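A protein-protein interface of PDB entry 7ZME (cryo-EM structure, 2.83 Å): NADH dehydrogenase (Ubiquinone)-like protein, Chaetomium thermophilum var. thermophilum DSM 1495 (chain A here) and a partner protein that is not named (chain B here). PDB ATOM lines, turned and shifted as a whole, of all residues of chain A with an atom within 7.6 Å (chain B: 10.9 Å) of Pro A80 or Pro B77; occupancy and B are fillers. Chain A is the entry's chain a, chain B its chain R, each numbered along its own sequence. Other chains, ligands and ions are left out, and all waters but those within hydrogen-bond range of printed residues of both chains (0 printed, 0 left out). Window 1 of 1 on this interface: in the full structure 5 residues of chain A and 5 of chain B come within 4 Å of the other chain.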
ATOM      1  N   ARG A  75       6.122  15.551 -24.760  1.00  0.00           N
ATOM      2  CA  ARG A  75       6.753  14.433 -25.443  1.00  0.00           C
ATOM      3  C   ARG A  75       7.837  13.796 -24.583  1.00  0.00           C
ATOM      4  O   ARG A  75       8.474  12.828 -25.008  1.00  0.00           O
ATOM      5  CB  ARG A  75       7.292  14.913 -26.792  1.00  0.00           C
ATOM      6  CG  ARG A  75       7.477  13.812 -27.800  1.00  0.00           C
ATOM      7  CD  ARG A  75       7.823  14.357 -29.168  1.00  0.00           C
ATOM      8  NE  ARG A  75       6.836  15.308 -29.658  1.00  0.00           N
ATOM      9  CZ  ARG A  75       7.117  16.565 -29.979  1.00  0.00           C
ATOM     10  NH1 ARG A  75       6.160  17.371 -30.409  1.00  0.00           N
ATOM     11  NH2 ARG A  75       8.363  17.010 -29.895  1.00  0.00           N
ATOM     12  N   GLN A  76       8.038  14.337 -23.380  1.00  0.00           N
ATOM     13  CA  GLN A  76       8.842  13.710 -22.341  1.00  0.00           C
ATOM     14  C   GLN A  76       8.389  12.290 -22.033  1.00  0.00           C
ATOM     15  O   GLN A  76       9.212  11.436 -21.690  1.00  0.00           O
ATOM     16  CB  GLN A  76       8.750  14.571 -21.082  1.00  0.00           C
ATOM     17  CG  GLN A  76       9.241  13.936 -19.806  1.00  0.00           C
ATOM     18  CD  GLN A  76       8.958  14.810 -18.604  1.00  0.00           C
ATOM     19  OE1 GLN A  76       8.535  15.953 -18.745  1.00  0.00           O
ATOM     20  NE2 GLN A  76       9.144  14.260 -17.414  1.00  0.00           N
ATOM     21  N   PHE A  77       7.095  12.018 -22.148  1.00  0.00           N
ATOM     22  CA  PHE A  77       6.516  10.788 -21.640  1.00  0.00           C
ATOM     23  C   PHE A  77       6.429   9.685 -22.685  1.00  0.00           C
ATOM     24  O   PHE A  77       5.849   8.632 -22.404  1.00  0.00           O
ATOM     25  CB  PHE A  77       5.132  11.076 -21.061  1.00  0.00           C
ATOM     26  CG  PHE A  77       5.138  12.145 -20.012  1.00  0.00           C
ATOM     27  CD1 PHE A  77       5.769  11.937 -18.799  1.00  0.00           C
ATOM     28  CD2 PHE A  77       4.524  13.361 -20.241  1.00  0.00           C
ATOM     29  CE1 PHE A  77       5.781  12.921 -17.831  1.00  0.00           C
ATOM     30  CE2 PHE A  77       4.531  14.348 -19.278  1.00  0.00           C
ATOM     31  CZ  PHE A  77       5.161  14.128 -18.071  1.00  0.00           C
ATOM     32  N   ARG A  78       6.982   9.895 -23.873  1.00  0.00           N
ATOM     33  CA  ARG A  78       7.082   8.813 -24.833  1.00  0.00           C
ATOM     34  C   ARG A  78       8.272   7.919 -24.498  1.00  0.00           C
ATOM     35  O   ARG A  78       9.117   8.244 -23.662  1.00  0.00           O
ATOM     36  CB  ARG A  78       7.212   9.358 -26.250  1.00  0.00           C
ATOM     37  CG  ARG A  78       6.024  10.163 -26.712  1.00  0.00           C
ATOM     38  CD  ARG A  78       6.146  10.454 -28.185  1.00  0.00           C
ATOM     39  NE  ARG A  78       5.133  11.384 -28.660  1.00  0.00           N
ATOM     40  CZ  ARG A  78       5.132  11.901 -29.881  1.00  0.00           C
ATOM     41  NH1 ARG A  78       4.179  12.745 -30.251  1.00  0.00           N
ATOM     42  NH2 ARG A  78       6.092  11.574 -30.733  1.00  0.00           N
ATOM     43  N   ASP A  79       8.331   6.778 -25.162  1.00  0.00           N
ATOM     44  CA  ASP A  79       9.395   5.819 -24.909  1.00  0.00           C
ATOM     45  C   ASP A  79      10.708   6.329 -25.484  1.00  0.00           C
ATOM     46  O   ASP A  79      10.785   6.591 -26.691  1.00  0.00           O
ATOM     47  CB  ASP A  79       9.043   4.469 -25.522  1.00  0.00           C
ATOM     48  CG  ASP A  79      10.027   3.381 -25.146  1.00  0.00           C
ATOM     49  OD1 ASP A  79      10.853   3.604 -24.240  1.00  0.00           O
ATOM     50  OD2 ASP A  79       9.967   2.293 -25.753  1.00  0.00           O
ATOM     51  N   PRO A  80      11.751   6.501 -24.672  1.00  0.00           N
ATOM     52  CA  PRO A  80      13.071   6.795 -25.242  1.00  0.00           C
ATOM     53  C   PRO A  80      13.594   5.678 -26.115  1.00  0.00           C
ATOM     54  O   PRO A  80      14.329   5.938 -27.075  1.00  0.00           O
ATOM     55  CB  PRO A  80      13.949   7.001 -24.002  1.00  0.00           C
ATOM     56  CG  PRO A  80      13.004   7.227 -22.878  1.00  0.00           C
ATOM     57  CD  PRO A  80      11.776   6.469 -23.202  1.00  0.00           C
ATOM     58  N   HIS A  81      13.230   4.436 -25.811  1.00  0.00           N
ATOM     59  CA  HIS A  81      13.783   3.266 -26.471  1.00  0.00           C
ATOM     60  C   HIS A  81      12.948   2.793 -27.649  1.00  0.00           C
ATOM     61  O   HIS A  81      13.285   1.772 -28.256  1.00  0.00           O
ATOM     62  CB  HIS A  81      13.939   2.132 -25.458  1.00  0.00           C
ATOM     63  CG  HIS A  81      14.915   2.436 -24.367  1.00  0.00           C
ATOM     64  ND1 HIS A  81      14.552   2.494 -23.039  1.00  0.00           N
ATOM     65  CD2 HIS A  81      16.240   2.708 -24.408  1.00  0.00           C
ATOM     66  CE1 HIS A  81      15.613   2.782 -22.308  1.00  0.00           C
ATOM     67  NE2 HIS A  81      16.650   2.916 -23.114  1.00  0.00           N
ATOM     68  N   ALA A  82      11.878   3.501 -27.990  1.00  0.00           N
ATOM     69  CA  ALA A  82      11.096   3.145 -29.160  1.00  0.00           C
ATOM     70  C   ALA A  82      11.829   3.558 -30.429  1.00  0.00           C
ATOM     71  O   ALA A  82      12.770   4.355 -30.406  1.00  0.00           O
ATOM     72  CB  ALA A  82       9.719   3.803 -29.114  1.00  0.00           C
ATOM     73  N   ASP A  83      11.398   2.989 -31.549  1.00  0.00           N
ATOM     74  CA  ASP A  83      11.933   3.393 -32.843  1.00  0.00           C
ATOM     75  C   ASP A  83      11.345   4.746 -33.213  1.00  0.00           C
ATOM     76  O   ASP A  83      10.134   4.874 -33.414  1.00  0.00           O
ATOM     77  CB  ASP A  83      11.616   2.343 -33.903  1.00  0.00           C
ATOM     78  CG  ASP A  83      12.380   1.052 -33.688  1.00  0.00           C
ATOM     79  OD1 ASP A  83      13.495   1.108 -33.129  1.00  0.00           O
ATOM     80  OD2 ASP A  83      11.867  -0.017 -34.079  1.00  0.00           O
ATOM     81  N   TRP A  84      12.197   5.760 -33.292  1.00  0.00           N
ATOM     82  CA  TRP A  84      11.781   7.115 -33.608  1.00  0.00           C
ATOM     83  C   TRP A  84      12.529   7.597 -34.840  1.00  0.00           C
ATOM     84  O   TRP A  84      13.731   7.358 -34.979  1.00  0.00           O
ATOM     85  CB  TRP A  84      12.049   8.064 -32.440  1.00  0.00           C
ATOM     86  CG  TRP A  84      11.283   7.741 -31.196  1.00  0.00           C
ATOM     87  CD1 TRP A  84      11.798   7.341 -30.001  1.00  0.00           C
ATOM     88  CD2 TRP A  84       9.863   7.792 -31.024  1.00  0.00           C
ATOM     89  NE1 TRP A  84      10.790   7.139 -29.097  1.00  0.00           N
ATOM     90  CE2 TRP A  84       9.591   7.409 -29.699  1.00  0.00           C
ATOM     91  CE3 TRP A  84       8.796   8.125 -31.862  1.00  0.00           C
ATOM     92  CZ2 TRP A  84       8.299   7.350 -29.192  1.00  0.00           C
ATOM     93  CZ3 TRP A  84       7.516   8.065 -31.356  1.00  0.00           C
ATOM     94  CH2 TRP A  84       7.277   7.680 -30.036  1.00  0.00           C
ATOM     95  N   LYS A  87      15.039  10.464 -32.953  1.00  0.00           N
ATOM     96  CA  LYS A  87      15.229   9.878 -31.632  1.00  0.00           C
ATOM     97  C   LYS A  87      15.365  10.954 -30.562  1.00  0.00           C
ATOM     98  O   LYS A  87      14.831  10.813 -29.457  1.00  0.00           O
ATOM     99  CB  LYS A  87      16.450   8.960 -31.633  1.00  0.00           C
ATOM    100  CG  LYS A  87      16.648   8.202 -30.331  1.00  0.00           C
ATOM    101  CD  LYS A  87      17.909   7.358 -30.366  1.00  0.00           C
ATOM    102  CE  LYS A  87      17.730   6.136 -31.251  1.00  0.00           C
ATOM    103  NZ  LYS A  87      18.914   5.238 -31.204  1.00  0.00           N
ATOM    104  N   GLN A  88      16.080  12.036 -30.876  1.00  0.00           N
ATOM    105  CA  GLN A  88      16.244  13.125 -29.920  1.00  0.00           C
ATOM    106  C   GLN A  88      14.908  13.754 -29.563  1.00  0.00           C
ATOM    107  O   GLN A  88      14.642  14.046 -28.393  1.00  0.00           O
ATOM    108  CB  GLN A  88      17.185  14.181 -30.489  1.00  0.00           C
ATOM    109  CG  GLN A  88      18.616  14.060 -30.029  1.00  0.00           C
ATOM    110  CD  GLN A  88      19.369  15.348 -30.216  1.00  0.00           C
ATOM    111  OE1 GLN A  88      19.396  15.906 -31.311  1.00  0.00           O
ATOM    112  NE2 GLN A  88      19.978  15.838 -29.146  1.00  0.00           N
ATOM    113  N   ARG A  90      11.931  12.262 -30.156  1.00  0.00           N
ATOM    114  CA  ARG A  90      10.976  11.184 -29.875  1.00  0.00           C
ATOM    115  C   ARG A  90       9.690  11.364 -30.683  1.00  0.00           C
ATOM    116  O   ARG A  90       8.583  11.411 -30.146  1.00  0.00           O
ATOM    117  CB  ARG A  90      10.668  11.083 -28.378  1.00  0.00           C
ATOM    118  CG  ARG A  90      11.888  10.971 -27.493  1.00  0.00           C
ATOM    119  CD  ARG A  90      11.585  10.116 -26.293  1.00  0.00           C
ATOM    120  NE  ARG A  90      12.602  10.240 -25.263  1.00  0.00           N
ATOM    121  CZ  ARG A  90      12.331  10.488 -23.988  1.00  0.00           C
ATOM    122  NH1 ARG A  90      11.074  10.638 -23.594  1.00  0.00           N
ATOM    123  NH2 ARG A  90      13.315  10.589 -23.108  1.00  0.00           N
ATOM    124  N   MET A 106      10.710  17.897 -26.560  1.00  0.00           N
ATOM    125  CA  MET A 106      11.731  17.535 -25.582  1.00  0.00           C
ATOM    126  C   MET A 106      12.396  18.769 -24.985  1.00  0.00           C
ATOM    127  O   MET A 106      12.647  18.818 -23.775  1.00  0.00           O
ATOM    128  CB  MET A 106      12.773  16.615 -26.218  1.00  0.00           C
ATOM    129  CG  MET A 106      12.248  15.238 -26.590  1.00  0.00           C
ATOM    130  SD  MET A 106      11.354  14.401 -25.270  1.00  0.00           S
ATOM    131  CE  MET A 106      12.620  14.280 -24.013  1.00  0.00           C
ATOM    132  N   LYS B  16      14.799  -3.827 -10.081  1.00  0.00           N
ATOM    133  CA  LYS B  16      15.475  -2.531 -10.338  1.00  0.00           C
ATOM    134  C   LYS B  16      15.126  -1.541  -9.238  1.00  0.00           C
ATOM    135  O   LYS B  16      16.026  -0.825  -8.809  1.00  0.00           O
ATOM    136  CB  LYS B  16      15.111  -2.010 -11.726  1.00  0.00           C
ATOM    137  CG  LYS B  16      15.926  -2.596 -12.870  1.00  0.00           C
ATOM    138  CD  LYS B  16      15.698  -1.890 -14.187  1.00  0.00           C
ATOM    139  CE  LYS B  16      16.123  -0.437 -14.156  1.00  0.00           C
ATOM    140  NZ  LYS B  16      15.901   0.231 -15.458  1.00  0.00           N
ATOM    141  N   PRO B  70      15.449   7.069 -10.195  1.00  0.00           N
ATOM    142  CA  PRO B  70      16.111   5.783 -10.426  1.00  0.00           C
ATOM    143  C   PRO B  70      17.500   5.855 -11.068  1.00  0.00           C
ATOM    144  O   PRO B  70      17.790   6.835 -11.706  1.00  0.00           O
ATOM    145  CB  PRO B  70      15.200   5.095 -11.444  1.00  0.00           C
ATOM    146  CG  PRO B  70      13.878   5.776 -11.279  1.00  0.00           C
ATOM    147  CD  PRO B  70      14.293   7.214 -11.100  1.00  0.00           C
ATOM    148  N   TYR B  71      18.315   4.820 -10.896  1.00  0.00           N
ATOM    149  CA  TYR B  71      19.647   4.792 -11.556  1.00  0.00           C
ATOM    150  C   TYR B  71      19.502   4.699 -13.081  1.00  0.00           C
ATOM    151  O   TYR B  71      18.616   3.976 -13.564  1.00  0.00           O
ATOM    152  CB  TYR B  71      20.571   3.713 -10.985  1.00  0.00           C
ATOM    153  CG  TYR B  71      21.719   3.348 -11.888  1.00  0.00           C
ATOM    154  CD1 TYR B  71      22.922   4.026 -11.822  1.00  0.00           C
ATOM    155  CD2 TYR B  71      21.591   2.343 -12.828  1.00  0.00           C
ATOM    156  CE1 TYR B  71      23.976   3.709 -12.661  1.00  0.00           C
ATOM    157  CE2 TYR B  71      22.635   2.010 -13.673  1.00  0.00           C
ATOM    158  CZ  TYR B  71      23.832   2.696 -13.591  1.00  0.00           C
ATOM    159  OH  TYR B  71      24.867   2.375 -14.418  1.00  0.00           O
ATOM    160  N   CYS B  72      20.365   5.401 -13.807  1.00  0.00           N
ATOM    161  CA  CYS B  72      20.335   5.404 -15.284  1.00  0.00           C
ATOM    162  C   CYS B  72      21.789   5.482 -15.773  1.00  0.00           C
ATOM    163  O   CYS B  72      22.436   6.502 -15.503  1.00  0.00           O
ATOM    164  CB  CYS B  72      19.572   6.609 -15.815  1.00  0.00           C
ATOM    165  SG  CYS B  72      19.012   6.430 -17.527  1.00  0.00           S
ATOM    166  N   PRO B  73      22.358   4.452 -16.441  1.00  0.00           N
ATOM    167  CA  PRO B  73      23.754   4.499 -16.892  1.00  0.00           C
ATOM    168  C   PRO B  73      24.021   5.751 -17.708  1.00  0.00           C
ATOM    169  O   PRO B  73      23.120   6.261 -18.390  1.00  0.00           O
ATOM    170  CB  PRO B  73      23.897   3.227 -17.745  1.00  0.00           C
ATOM    171  CG  PRO B  73      22.517   2.722 -17.954  1.00  0.00           C
ATOM    172  CD  PRO B  73      21.691   3.201 -16.822  1.00  0.00           C
ATOM    173  N   PRO B  74      25.243   6.284 -17.655  1.00  0.00           N
ATOM    174  CA  PRO B  74      25.493   7.610 -18.247  1.00  0.00           C
ATOM    175  C   PRO B  74      25.175   7.696 -19.727  1.00  0.00           C
ATOM    176  O   PRO B  74      24.762   8.759 -20.201  1.00  0.00           O
ATOM    177  CB  PRO B  74      26.986   7.834 -17.979  1.00  0.00           C
ATOM    178  CG  PRO B  74      27.313   6.920 -16.840  1.00  0.00           C
ATOM    179  CD  PRO B  74      26.447   5.722 -17.021  1.00  0.00           C
ATOM    180  N   THR B  75      25.356   6.611 -20.474  1.00  0.00           N
ATOM    181  CA  THR B  75      25.058   6.614 -21.898  1.00  0.00           C
ATOM    182  C   THR B  75      23.593   6.333 -22.200  1.00  0.00           C
ATOM    183  O   THR B  75      23.165   6.531 -23.340  1.00  0.00           O
ATOM    184  CB  THR B  75      25.933   5.584 -22.609  1.00  0.00           C
ATOM    185  OG1 THR B  75      25.662   4.284 -22.075  1.00  0.00           O
ATOM    186  CG2 THR B  75      27.400   5.910 -22.398  1.00  0.00           C
ATOM    187  N   ALA B  76      22.824   5.886 -21.217  1.00  0.00           N
ATOM    188  CA  ALA B  76      21.414   5.597 -21.404  1.00  0.00           C
ATOM    189  C   ALA B  76      20.608   6.884 -21.519  1.00  0.00           C
ATOM    190  O   ALA B  76      21.037   7.938 -21.050  1.00  0.00           O
ATOM    191  CB  ALA B  76      20.896   4.763 -20.241  1.00  0.00           C
ATOM    192  N   PRO B  77      19.434   6.828 -22.146  1.00  0.00           N
ATOM    193  CA  PRO B  77      18.577   8.021 -22.202  1.00  0.00           C
ATOM    194  C   PRO B  77      18.176   8.461 -20.803  1.00  0.00           C
ATOM    195  O   PRO B  77      17.493   7.739 -20.074  1.00  0.00           O
ATOM    196  CB  PRO B  77      17.371   7.553 -23.024  1.00  0.00           C
ATOM    197  CG  PRO B  77      17.864   6.384 -23.795  1.00  0.00           C
ATOM    198  CD  PRO B  77      18.868   5.710 -22.916  1.00  0.00           C
ATOM    199  N   GLY B  78      18.608   9.660 -20.433  1.00  0.00           N
ATOM    200  CA  GLY B  78      18.475  10.146 -19.082  1.00  0.00           C
ATOM    201  C   GLY B  78      19.750  10.079 -18.273  1.00  0.00           C
ATOM    202  O   GLY B  78      19.806  10.665 -17.185  1.00  0.00           O
ATOM    203  N   GLY B  79      20.772   9.383 -18.768  1.00  0.00           N
ATOM    204  CA  GLY B  79      22.053   9.361 -18.104  1.00  0.00           C
ATOM    205  C   GLY B  79      22.815  10.654 -18.291  1.00  0.00           C
ATOM    206  O   GLY B  79      22.449  11.516 -19.081  1.00  0.00           O
ATOM    207  N   SER B  80      23.912  10.774 -17.546  1.00  0.00           N
ATOM    208  CA  SER B  80      24.658  12.028 -17.508  1.00  0.00           C
ATOM    209  C   SER B  80      25.400  12.307 -18.809  1.00  0.00           C
ATOM    210  O   SER B  80      25.528  13.467 -19.207  1.00  0.00           O
ATOM    211  CB  SER B  80      25.636  12.008 -16.339  1.00  0.00           C
ATOM    212  OG  SER B  80      24.967  11.739 -15.124  1.00  0.00           O
ATOM    213  N   LYS B  81      25.905  11.271 -19.471  1.00  0.00           N
ATOM    214  CA  LYS B  81      26.732  11.417 -20.659  1.00  0.00           C
ATOM    215  C   LYS B  81      25.928  11.296 -21.951  1.00  0.00           C
ATOM    216  O   LYS B  81      26.507  11.317 -23.039  1.00  0.00           O
ATOM    217  CB  LYS B  81      27.852  10.368 -20.622  1.00  0.00           C
ATOM    218  CG  LYS B  81      28.963  10.543 -21.635  1.00  0.00           C
ATOM    219  CD  LYS B  81      29.782   9.280 -21.762  1.00  0.00           C
ATOM    220  CE  LYS B  81      31.194   9.483 -21.272  1.00  0.00           C
ATOM    221  NZ  LYS B  81      32.113   8.435 -21.790  1.00  0.00           N
ATOM    222  N   TYR B  82      24.607  11.200 -21.856  1.00  0.00           N
ATOM    223  CA  TYR B  82      23.784  10.867 -23.008  1.00  0.00           C
ATOM    224  C   TYR B  82      23.602  12.083 -23.913  1.00  0.00           C
ATOM    225  O   TYR B  82      23.291  13.179 -23.445  1.00  0.00           O
ATOM    226  CB  TYR B  82      22.437  10.337 -22.520  1.00  0.00           C
ATOM    227  CG  TYR B  82      21.318  10.338 -23.526  1.00  0.00           C
ATOM    228  CD1 TYR B  82      21.404   9.580 -24.684  1.00  0.00           C
ATOM    229  CD2 TYR B  82      20.161  11.063 -23.305  1.00  0.00           C
ATOM    230  CE1 TYR B  82      20.382   9.558 -25.598  1.00  0.00           C
ATOM    231  CE2 TYR B  82      19.135  11.049 -24.217  1.00  0.00           C
ATOM    232  CZ  TYR B  82      19.250  10.295 -25.361  1.00  0.00           C
ATOM    233  OH  TYR B  82      18.225  10.283 -26.276  1.00  0.00           O
ATOM    234  N   GLU B  83      23.809  11.881 -25.216  1.00  0.00           N
ATOM    235  CA  GLU B  83      23.719  12.936 -26.234  1.00  0.00           C
ATOM    236  C   GLU B  83      24.799  13.997 -26.050  1.00  0.00           C
ATOM    237  O   GLU B  83      24.624  15.162 -26.403  1.00  0.00           O
ATOM    238  CB  GLU B  83      22.338  13.591 -26.241  1.00  0.00           C
ATOM    239  CG  GLU B  83      21.204  12.709 -26.686  1.00  0.00           C
ATOM    240  CD  GLU B  83      19.865  13.422 -26.641  1.00  0.00           C
ATOM    241  OE1 GLU B  83      19.810  14.564 -26.141  1.00  0.00           O
ATOM    242  OE2 GLU B  83      18.861  12.832 -27.089  1.00  0.00           O
ATOM    243  N   ARG B  84      25.945  13.584 -25.508  1.00  0.00           N
ATOM    244  CA  ARG B  84      26.940  14.575 -25.113  1.00  0.00           C
ATOM    245  C   ARG B  84      27.691  15.136 -26.314  1.00  0.00           C
ATOM    246  O   ARG B  84      27.700  16.352 -26.535  1.00  0.00           O
ATOM    247  CB  ARG B  84      27.919  13.980 -24.102  1.00  0.00           C
ATOM    248  CG  ARG B  84      29.145  14.842 -23.888  1.00  0.00           C
ATOM    249  CD  ARG B  84      30.056  14.267 -22.835  1.00  0.00           C
ATOM    250  NE  ARG B  84      29.415  14.278 -21.525  1.00  0.00           N
ATOM    251  CZ  ARG B  84      30.039  14.015 -20.386  1.00  0.00           C
ATOM    252  NH1 ARG B  84      31.329  13.726 -20.391  1.00  0.00           N
ATOM    253  NH2 ARG B  84      29.374  14.047 -19.243  1.00  0.00           N
ATOM    254  N   LEU B  86      27.236  14.257 -29.731  1.00  0.00           N
ATOM    255  CA  LEU B  86      26.568  13.637 -30.863  1.00  0.00           C
ATOM    256  C   LEU B  86      27.220  14.061 -32.177  1.00  0.00           C
ATOM    257  O   LEU B  86      27.448  15.260 -32.392  1.00  0.00           O
ATOM    258  CB  LEU B  86      25.089  14.025 -30.885  1.00  0.00           C
ATOM    259  CG  LEU B  86      24.105  13.283 -29.988  1.00  0.00           C
ATOM    260  CD1 LEU B  86      22.783  14.027 -29.954  1.00  0.00           C
ATOM    261  CD2 LEU B  86      23.909  11.864 -30.472  1.00  0.00           C
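Pro A80 touches just one residue of chain B: Pro B77. Pro B77 touches just these residues of chain A: Pro A80 and His A81. Of chain B, only Pro B77 comes within 4 Å of His A81. No residue of chain B comes within 4 Å of Ala A82. Of the printed residues of chain A, Glu B83 touches Gln A88 (3.2 Å). Printed residues of chain A within 4 Å of Leu B86: Gln A88 (3.4 Å). Of the printed residues of chain B, Gln A88 touches Glu B83 (3.2 Å) and Leu B86 (3.4 Å). Ala B76 touches none of the printed residues of chain A. The nearest residue of chain B that does not touch Pro A80 is Tyr B82 (5.9 Å). The nearest residue of chain A that does not touch Pro B77 is Arg A90 (5.1 Å).
SG of Cys B72 lies within hydrogen-bond range of O of Pro B77, 3.2 Å away. OE2 of Glu B83 is in hydrogen-bond range of OH of Tyr B82 (2.8 Å). OD1 of Asp A79 lies within hydrogen-bond range of N of His A81 (3.0 Å).
Pro B77 touches Pro A80 (CB to CB, 3.6 Å). NE2 of His A81 touches CD of Pro B77, 3.6 Å away. CD1 of Leu B86 touches NE2 of Gln A88 (3.4 Å).
OE1 of Glu B83 sits at hydrogen-bond distance from NE2 of Gln A88 (3.3 Å).
Hydrophobic or aromatic side chains of chain A that line the printed part of chain B: Pro A80 and His A81. Of the 17 printed residues of chain B, 3 touch a printed residue of chain A. Printed residues of chain B that touch a printed residue of chain A: Pro B77, Glu B83 and Leu B86. Hydrophobic or aromatic side chains of chain B that line the printed part of chain A: Pro B77 and Leu B86. Among the printed residues, no Asp or Glu carboxylate lies within 4 Å of a Lys or Arg side-chain nitrogen of the other chain.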
